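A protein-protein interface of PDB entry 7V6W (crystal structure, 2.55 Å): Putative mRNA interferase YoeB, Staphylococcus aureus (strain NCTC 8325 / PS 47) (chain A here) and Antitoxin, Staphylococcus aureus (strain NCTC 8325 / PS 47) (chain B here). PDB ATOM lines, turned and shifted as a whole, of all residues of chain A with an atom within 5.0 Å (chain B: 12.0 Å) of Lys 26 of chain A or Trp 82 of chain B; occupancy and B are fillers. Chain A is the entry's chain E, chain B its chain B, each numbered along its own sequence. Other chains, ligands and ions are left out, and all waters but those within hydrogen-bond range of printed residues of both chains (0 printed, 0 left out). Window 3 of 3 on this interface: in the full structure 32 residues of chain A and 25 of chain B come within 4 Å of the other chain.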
ATOM      1  N   LEU A  17      -8.732  24.392  16.952  1.00  0.00           N
ATOM      2  CA  LEU A  17      -8.003  25.004  18.056  1.00  0.00           C
ATOM      3  C   LEU A  17      -7.378  23.960  18.971  1.00  0.00           C
ATOM      4  O   LEU A  17      -6.335  24.219  19.581  1.00  0.00           O
ATOM      5  CB  LEU A  17      -8.930  25.925  18.849  1.00  0.00           C
ATOM      6  CG  LEU A  17      -9.513  27.090  18.047  1.00  0.00           C
ATOM      7  CD1 LEU A  17     -10.366  27.989  18.930  1.00  0.00           C
ATOM      8  CD2 LEU A  17      -8.399  27.883  17.377  1.00  0.00           C
ATOM      9  N   ILE A  20      -4.239  23.036  17.383  1.00  0.00           N
ATOM     10  CA  ILE A  20      -3.286  24.132  17.525  1.00  0.00           C
ATOM     11  C   ILE A  20      -2.602  24.069  18.883  1.00  0.00           C
ATOM     12  O   ILE A  20      -1.380  24.235  18.988  1.00  0.00           O
ATOM     13  CB  ILE A  20      -3.998  25.481  17.312  1.00  0.00           C
ATOM     14  CG1 ILE A  20      -4.390  25.656  15.844  1.00  0.00           C
ATOM     15  CG2 ILE A  20      -3.122  26.634  17.777  1.00  0.00           C
ATOM     16  CD1 ILE A  20      -3.210  25.671  14.897  1.00  0.00           C
ATOM     17  N   LYS A  21      -3.376  23.822  19.942  1.00  0.00           N
ATOM     18  CA  LYS A  21      -2.817  23.759  21.288  1.00  0.00           C
ATOM     19  C   LYS A  21      -1.794  22.636  21.409  1.00  0.00           C
ATOM     20  O   LYS A  21      -0.668  22.853  21.875  1.00  0.00           O
ATOM     21  CB  LYS A  21      -3.944  23.575  22.305  1.00  0.00           C
ATOM     22  CG  LYS A  21      -3.481  23.261  23.715  1.00  0.00           C
ATOM     23  CD  LYS A  21      -4.670  22.979  24.623  1.00  0.00           C
ATOM     24  CE  LYS A  21      -4.223  22.606  26.026  1.00  0.00           C
ATOM     25  NZ  LYS A  21      -5.382  22.299  26.909  1.00  0.00           N
ATOM     26  N   TYR A  24       1.581  23.233  19.906  1.00  0.00           N
ATOM     27  CA  TYR A  24       2.320  24.378  20.441  1.00  0.00           C
ATOM     28  C   TYR A  24       2.316  25.550  19.462  1.00  0.00           C
ATOM     29  O   TYR A  24       3.303  26.275  19.323  1.00  0.00           O
ATOM     30  CB  TYR A  24       3.750  23.987  20.823  1.00  0.00           C
ATOM     31  CG  TYR A  24       3.813  22.848  21.813  1.00  0.00           C
ATOM     32  CD1 TYR A  24       4.101  21.555  21.395  1.00  0.00           C
ATOM     33  CD2 TYR A  24       3.571  23.061  23.164  1.00  0.00           C
ATOM     34  CE1 TYR A  24       4.154  20.509  22.297  1.00  0.00           C
ATOM     35  CE2 TYR A  24       3.621  22.021  24.073  1.00  0.00           C
ATOM     36  CZ  TYR A  24       3.914  20.747  23.633  1.00  0.00           C
ATOM     37  OH  TYR A  24       3.966  19.708  24.532  1.00  0.00           O
ATOM     38  N   LEU A  25       1.190  25.733  18.773  1.00  0.00           N
ATOM     39  CA  LEU A  25       0.988  26.860  17.873  1.00  0.00           C
ATOM     40  C   LEU A  25       0.050  27.902  18.462  1.00  0.00           C
ATOM     41  O   LEU A  25      -0.293  28.872  17.778  1.00  0.00           O
ATOM     42  CB  LEU A  25       0.450  26.376  16.526  1.00  0.00           C
ATOM     43  CG  LEU A  25       1.322  25.376  15.770  1.00  0.00           C
ATOM     44  CD1 LEU A  25       0.673  24.999  14.450  1.00  0.00           C
ATOM     45  CD2 LEU A  25       2.710  25.951  15.548  1.00  0.00           C
ATOM     46  N   LYS A  26      -0.378  27.718  19.715  1.00  0.00           N
ATOM     47  CA  LYS A  26      -1.317  28.649  20.328  1.00  0.00           C
ATOM     48  C   LYS A  26      -0.753  30.062  20.366  1.00  0.00           C
ATOM     49  O   LYS A  26      -1.479  31.035  20.131  1.00  0.00           O
ATOM     50  CB  LYS A  26      -1.672  28.174  21.738  1.00  0.00           C
ATOM     51  CG  LYS A  26      -2.534  29.142  22.526  1.00  0.00           C
ATOM     52  CD  LYS A  26      -2.582  28.754  23.994  1.00  0.00           C
ATOM     53  CE  LYS A  26      -3.284  29.815  24.824  1.00  0.00           C
ATOM     54  NZ  LYS A  26      -3.199  29.518  26.281  1.00  0.00           N
ATOM     55  N   LYS A  27       0.544  30.194  20.650  1.00  0.00           N
ATOM     56  CA  LYS A  27       1.152  31.517  20.728  1.00  0.00           C
ATOM     57  C   LYS A  27       1.104  32.222  19.377  1.00  0.00           C
ATOM     58  O   LYS A  27       0.755  33.406  19.300  1.00  0.00           O
ATOM     59  CB  LYS A  27       2.592  31.397  21.229  1.00  0.00           C
ATOM     60  CG  LYS A  27       3.211  32.705  21.692  1.00  0.00           C
ATOM     61  CD  LYS A  27       4.284  33.189  20.730  1.00  0.00           C
ATOM     62  CE  LYS A  27       5.061  34.357  21.321  1.00  0.00           C
ATOM     63  NZ  LYS A  27       6.137  34.844  20.415  1.00  0.00           N
ATOM     64  N   SER A  28       1.434  31.507  18.299  1.00  0.00           N
ATOM     65  CA  SER A  28       1.395  32.111  16.971  1.00  0.00           C
ATOM     66  C   SER A  28      -0.036  32.406  16.536  1.00  0.00           C
ATOM     67  O   SER A  28      -0.287  33.405  15.851  1.00  0.00           O
ATOM     68  CB  SER A  28       2.085  31.197  15.959  1.00  0.00           C
ATOM     69  OG  SER A  28       1.971  31.721  14.647  1.00  0.00           O
ATOM     70  N   PHE A  29      -0.984  31.547  16.919  1.00  0.00           N
ATOM     71  CA  PHE A  29      -2.380  31.784  16.567  1.00  0.00           C
ATOM     72  C   PHE A  29      -2.914  33.042  17.240  1.00  0.00           C
ATOM     73  O   PHE A  29      -3.616  33.840  16.607  1.00  0.00           O
ATOM     74  CB  PHE A  29      -3.228  30.570  16.946  1.00  0.00           C
ATOM     75  CG  PHE A  29      -4.703  30.773  16.743  1.00  0.00           C
ATOM     76  CD1 PHE A  29      -5.258  30.689  15.476  1.00  0.00           C
ATOM     77  CD2 PHE A  29      -5.535  31.042  17.818  1.00  0.00           C
ATOM     78  CE1 PHE A  29      -6.616  30.876  15.287  1.00  0.00           C
ATOM     79  CE2 PHE A  29      -6.893  31.230  17.635  1.00  0.00           C
ATOM     80  CZ  PHE A  29      -7.434  31.147  16.368  1.00  0.00           C
ATOM     81  N   LEU A  30      -2.590  33.238  18.521  1.00  0.00           N
ATOM     82  CA  LEU A  30      -3.065  34.420  19.229  1.00  0.00           C
ATOM     83  C   LEU A  30      -2.459  35.700  18.668  1.00  0.00           C
ATOM     84  O   LEU A  30      -3.070  36.769  18.773  1.00  0.00           O
ATOM     85  CB  LEU A  30      -2.765  34.295  20.723  1.00  0.00           C
ATOM     86  CG  LEU A  30      -3.518  33.182  21.454  1.00  0.00           C
ATOM     87  CD1 LEU A  30      -3.181  33.182  22.937  1.00  0.00           C
ATOM     88  CD2 LEU A  30      -5.020  33.314  21.237  1.00  0.00           C
ATOM     89  N   THR B  75     -18.563  31.521  18.579  1.00  0.00           N
ATOM     90  CA  THR B  75     -17.959  31.789  19.877  1.00  0.00           C
ATOM     91  C   THR B  75     -16.900  32.870  19.722  1.00  0.00           C
ATOM     92  O   THR B  75     -16.036  32.776  18.843  1.00  0.00           O
ATOM     93  CB  THR B  75     -17.341  30.522  20.477  1.00  0.00           C
ATOM     94  OG1 THR B  75     -18.369  29.552  20.715  1.00  0.00           O
ATOM     95  CG2 THR B  75     -16.639  30.838  21.791  1.00  0.00           C
ATOM     96  N   ASN B  76     -16.978  33.898  20.566  1.00  0.00           N
ATOM     97  CA  ASN B  76     -15.932  34.909  20.604  1.00  0.00           C
ATOM     98  C   ASN B  76     -14.606  34.260  20.979  1.00  0.00           C
ATOM     99  O   ASN B  76     -14.541  33.428  21.887  1.00  0.00           O
ATOM    100  CB  ASN B  76     -16.285  36.008  21.607  1.00  0.00           C
ATOM    101  CG  ASN B  76     -15.330  37.186  21.544  1.00  0.00           C
ATOM    102  OD1 ASN B  76     -14.171  37.085  21.944  1.00  0.00           O
ATOM    103  ND2 ASN B  76     -15.818  38.316  21.048  1.00  0.00           N
ATOM    104  N   ILE B  77     -13.544  34.647  20.267  1.00  0.00           N
ATOM    105  CA  ILE B  77     -12.246  34.009  20.458  1.00  0.00           C
ATOM    106  C   ILE B  77     -11.699  34.248  21.859  1.00  0.00           C
ATOM    107  O   ILE B  77     -10.900  33.447  22.356  1.00  0.00           O
ATOM    108  CB  ILE B  77     -11.254  34.490  19.376  1.00  0.00           C
ATOM    109  CG1 ILE B  77     -10.029  33.577  19.325  1.00  0.00           C
ATOM    110  CG2 ILE B  77     -10.848  35.936  19.619  1.00  0.00           C
ATOM    111  CD1 ILE B  77     -10.359  32.140  18.984  1.00  0.00           C
ATOM    112  N   ASP B  78     -12.122  35.327  22.522  1.00  0.00           N
ATOM    113  CA  ASP B  78     -11.688  35.575  23.891  1.00  0.00           C
ATOM    114  C   ASP B  78     -12.348  34.631  24.887  1.00  0.00           C
ATOM    115  O   ASP B  78     -11.797  34.410  25.970  1.00  0.00           O
ATOM    116  CB  ASP B  78     -11.975  37.024  24.287  1.00  0.00           C
ATOM    117  CG  ASP B  78     -11.110  38.016  23.536  1.00  0.00           C
ATOM    118  OD1 ASP B  78     -10.164  37.577  22.848  1.00  0.00           O
ATOM    119  OD2 ASP B  78     -11.377  39.233  23.631  1.00  0.00           O
ATOM    120  N   ASP B  79     -13.509  34.075  24.550  1.00  0.00           N
ATOM    121  CA  ASP B  79     -14.225  33.162  25.429  1.00  0.00           C
ATOM    122  C   ASP B  79     -13.831  31.707  25.216  1.00  0.00           C
ATOM    123  O   ASP B  79     -14.491  30.813  25.756  1.00  0.00           O
ATOM    124  CB  ASP B  79     -15.735  33.325  25.241  1.00  0.00           C
ATOM    125  CG  ASP B  79     -16.223  34.708  25.625  1.00  0.00           C
ATOM    126  OD1 ASP B  79     -15.612  35.327  26.523  1.00  0.00           O
ATOM    127  OD2 ASP B  79     -17.217  35.177  25.030  1.00  0.00           O
ATOM    128  N   ILE B  80     -12.777  31.451  24.441  1.00  0.00           N
ATOM    129  CA  ILE B  80     -12.317  30.087  24.221  1.00  0.00           C
ATOM    130  C   ILE B  80     -11.666  29.561  25.493  1.00  0.00           C
ATOM    131  O   ILE B  80     -10.780  30.206  26.069  1.00  0.00           O
ATOM    132  CB  ILE B  80     -11.344  30.033  23.033  1.00  0.00           C
ATOM    133  CG1 ILE B  80     -12.077  30.335  21.723  1.00  0.00           C
ATOM    134  CG2 ILE B  80     -10.655  28.679  22.963  1.00  0.00           C
ATOM    135  CD1 ILE B  80     -13.124  29.305  21.355  1.00  0.00           C
ATOM    136  N   ASP B  81     -12.112  28.389  25.943  1.00  0.00           N
ATOM    137  CA  ASP B  81     -11.526  27.725  27.105  1.00  0.00           C
ATOM    138  C   ASP B  81     -10.429  26.800  26.597  1.00  0.00           C
ATOM    139  O   ASP B  81     -10.670  25.645  26.243  1.00  0.00           O
ATOM    140  CB  ASP B  81     -12.586  26.967  27.893  1.00  0.00           C
ATOM    141  CG  ASP B  81     -12.035  26.336  29.160  1.00  0.00           C
ATOM    142  OD1 ASP B  81     -10.900  26.677  29.557  1.00  0.00           O
ATOM    143  OD2 ASP B  81     -12.740  25.495  29.756  1.00  0.00           O
ATOM    144  N   TRP B  82      -9.201  27.322  26.560  1.00  0.00           N
ATOM    145  CA  TRP B  82      -8.079  26.562  26.025  1.00  0.00           C
ATOM    146  C   TRP B  82      -7.728  25.349  26.877  1.00  0.00           C
ATOM    147  O   TRP B  82      -7.122  24.404  26.363  1.00  0.00           O
ATOM    148  CB  TRP B  82      -6.855  27.467  25.878  1.00  0.00           C
ATOM    149  CG  TRP B  82      -6.950  28.426  24.727  1.00  0.00           C
ATOM    150  CD1 TRP B  82      -7.388  29.718  24.766  1.00  0.00           C
ATOM    151  CD2 TRP B  82      -6.598  28.164  23.363  1.00  0.00           C
ATOM    152  NE1 TRP B  82      -7.329  30.277  23.512  1.00  0.00           N
ATOM    153  CE2 TRP B  82      -6.848  29.343  22.633  1.00  0.00           C
ATOM    154  CE3 TRP B  82      -6.096  27.047  22.689  1.00  0.00           C
ATOM    155  CZ2 TRP B  82      -6.612  29.435  21.262  1.00  0.00           C
ATOM    156  CZ3 TRP B  82      -5.862  27.141  21.331  1.00  0.00           C
ATOM    157  CH2 TRP B  82      -6.120  28.326  20.632  1.00  0.00           C
ATOM    158  N   ASP B  83      -8.093  25.344  28.157  1.00  0.00           N
ATOM    159  CA  ASP B  83      -7.724  24.221  29.007  1.00  0.00           C
ATOM    160  C   ASP B  83      -8.595  22.995  28.779  1.00  0.00           C
ATOM    161  O   ASP B  83      -8.222  21.900  29.209  1.00  0.00           O
ATOM    162  CB  ASP B  83      -7.779  24.635  30.475  1.00  0.00           C
ATOM    163  CG  ASP B  83      -6.850  25.785  30.781  1.00  0.00           C
ATOM    164  OD1 ASP B  83      -6.065  26.159  29.883  1.00  0.00           O
ATOM    165  OD2 ASP B  83      -6.906  26.320  31.908  1.00  0.00           O
ATOM    166  N   ASN B  84      -9.733  23.145  28.108  1.00  0.00           N
ATOM    167  CA  ASN B  84     -10.613  22.020  27.851  1.00  0.00           C
ATOM    168  C   ASN B  84     -10.767  21.704  26.372  1.00  0.00           C
ATOM    169  O   ASN B  84     -11.400  20.697  26.033  1.00  0.00           O
ATOM    170  CB  ASN B  84     -11.987  22.270  28.483  1.00  0.00           C
ATOM    171  CG  ASN B  84     -11.959  22.120  29.992  1.00  0.00           C
ATOM    172  OD1 ASN B  84     -12.029  21.008  30.514  1.00  0.00           O
ATOM    173  ND2 ASN B  84     -11.842  23.238  30.701  1.00  0.00           N
ATOM    174  N   LEU B  85     -10.193  22.512  25.487  1.00  0.00           N
ATOM    175  CA  LEU B  85     -10.303  22.284  24.054  1.00  0.00           C
ATOM    176  C   LEU B  85      -9.200  23.015  23.297  1.00  0.00           C
ATOM    177  O   LEU B  85      -9.454  24.008  22.616  1.00  0.00           O
ATOM    178  CB  LEU B  85     -11.676  22.730  23.550  1.00  0.00           C
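NZ of Lys 21 of chain A sits at hydrogen-bond distance from O of Trp 82 of chain B (2.8 Å).
The side-chain carboxylate (OD1) of Asp 81 of chain B lies close to the backbone NH (N) of Asp 83 of chain B (3.4 Å).
Among the printed residues, merely in contact across the chains: Leu 17 of chain A with Trp 82 of chain B, Lys 21 of chain A with Asp 83 of chain B, Phe 29 of chain A with Ile 77 of chain B, Leu 17 of chain A with Ile 80 of chain B, Lys 26 of chain A with Trp 82 of chain B and Phe 29 of chain A with Trp 82 of chain B.
Of chain B, only Trp 82 (3.9 Å) comes within 4 Å of Lys 26 of chain A. Trp 82 of chain B touches just these residues of chain A: Leu 17, Lys 21, Lys 26 and Phe 29. Of the printed residues of chain B, Leu 17 of chain A touches Ile 80 (3.9 Å) and Trp 82 (3.4 Å). Of chain B, only Trp 82 and Asp 83 come within 4 Å of Lys 21 of chain A. No residue of chain B comes within 4 Å of Ser 28 of chain A. Phe 29 of chain A touches just these residues of chain B: Ile 77 (3.8 Å) and Trp 82 (3.95 Å). Of the printed residues of chain A, Asp 83 of chain B touches Lys 21 (3.7 Å). Printed residues of chain A within 4 Å of Ile 77 of chain B: Phe 29 (3.8 Å). Of the printed residues of chain A, Ile 80 of chain B touches Leu 17. The nearest residue of chain B that does not touch Lys 26 of chain A is Asp 83 of chain B (5.7 Å). The nearest residue of chain A that does not touch Trp 82 of chain B is Leu 30 of chain A (4.2 Å). The nearest printed residue of chain A that does not touch Ile 77 of chain B is Leu 17 of chain A (4.2 Å).
Of the 11 printed residues of chain B, 4 touch a printed residue of chain A. Hydrophobic or aromatic side chains of chain B that line the printed part of chain A: Ile 77, Ile 80 and Trp 82. Hydrophobic or aromatic side chains of chain A that line the printed part of chain B: Leu 17 and Phe 29. Among the printed residues, 7 pairs touch across the chains.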
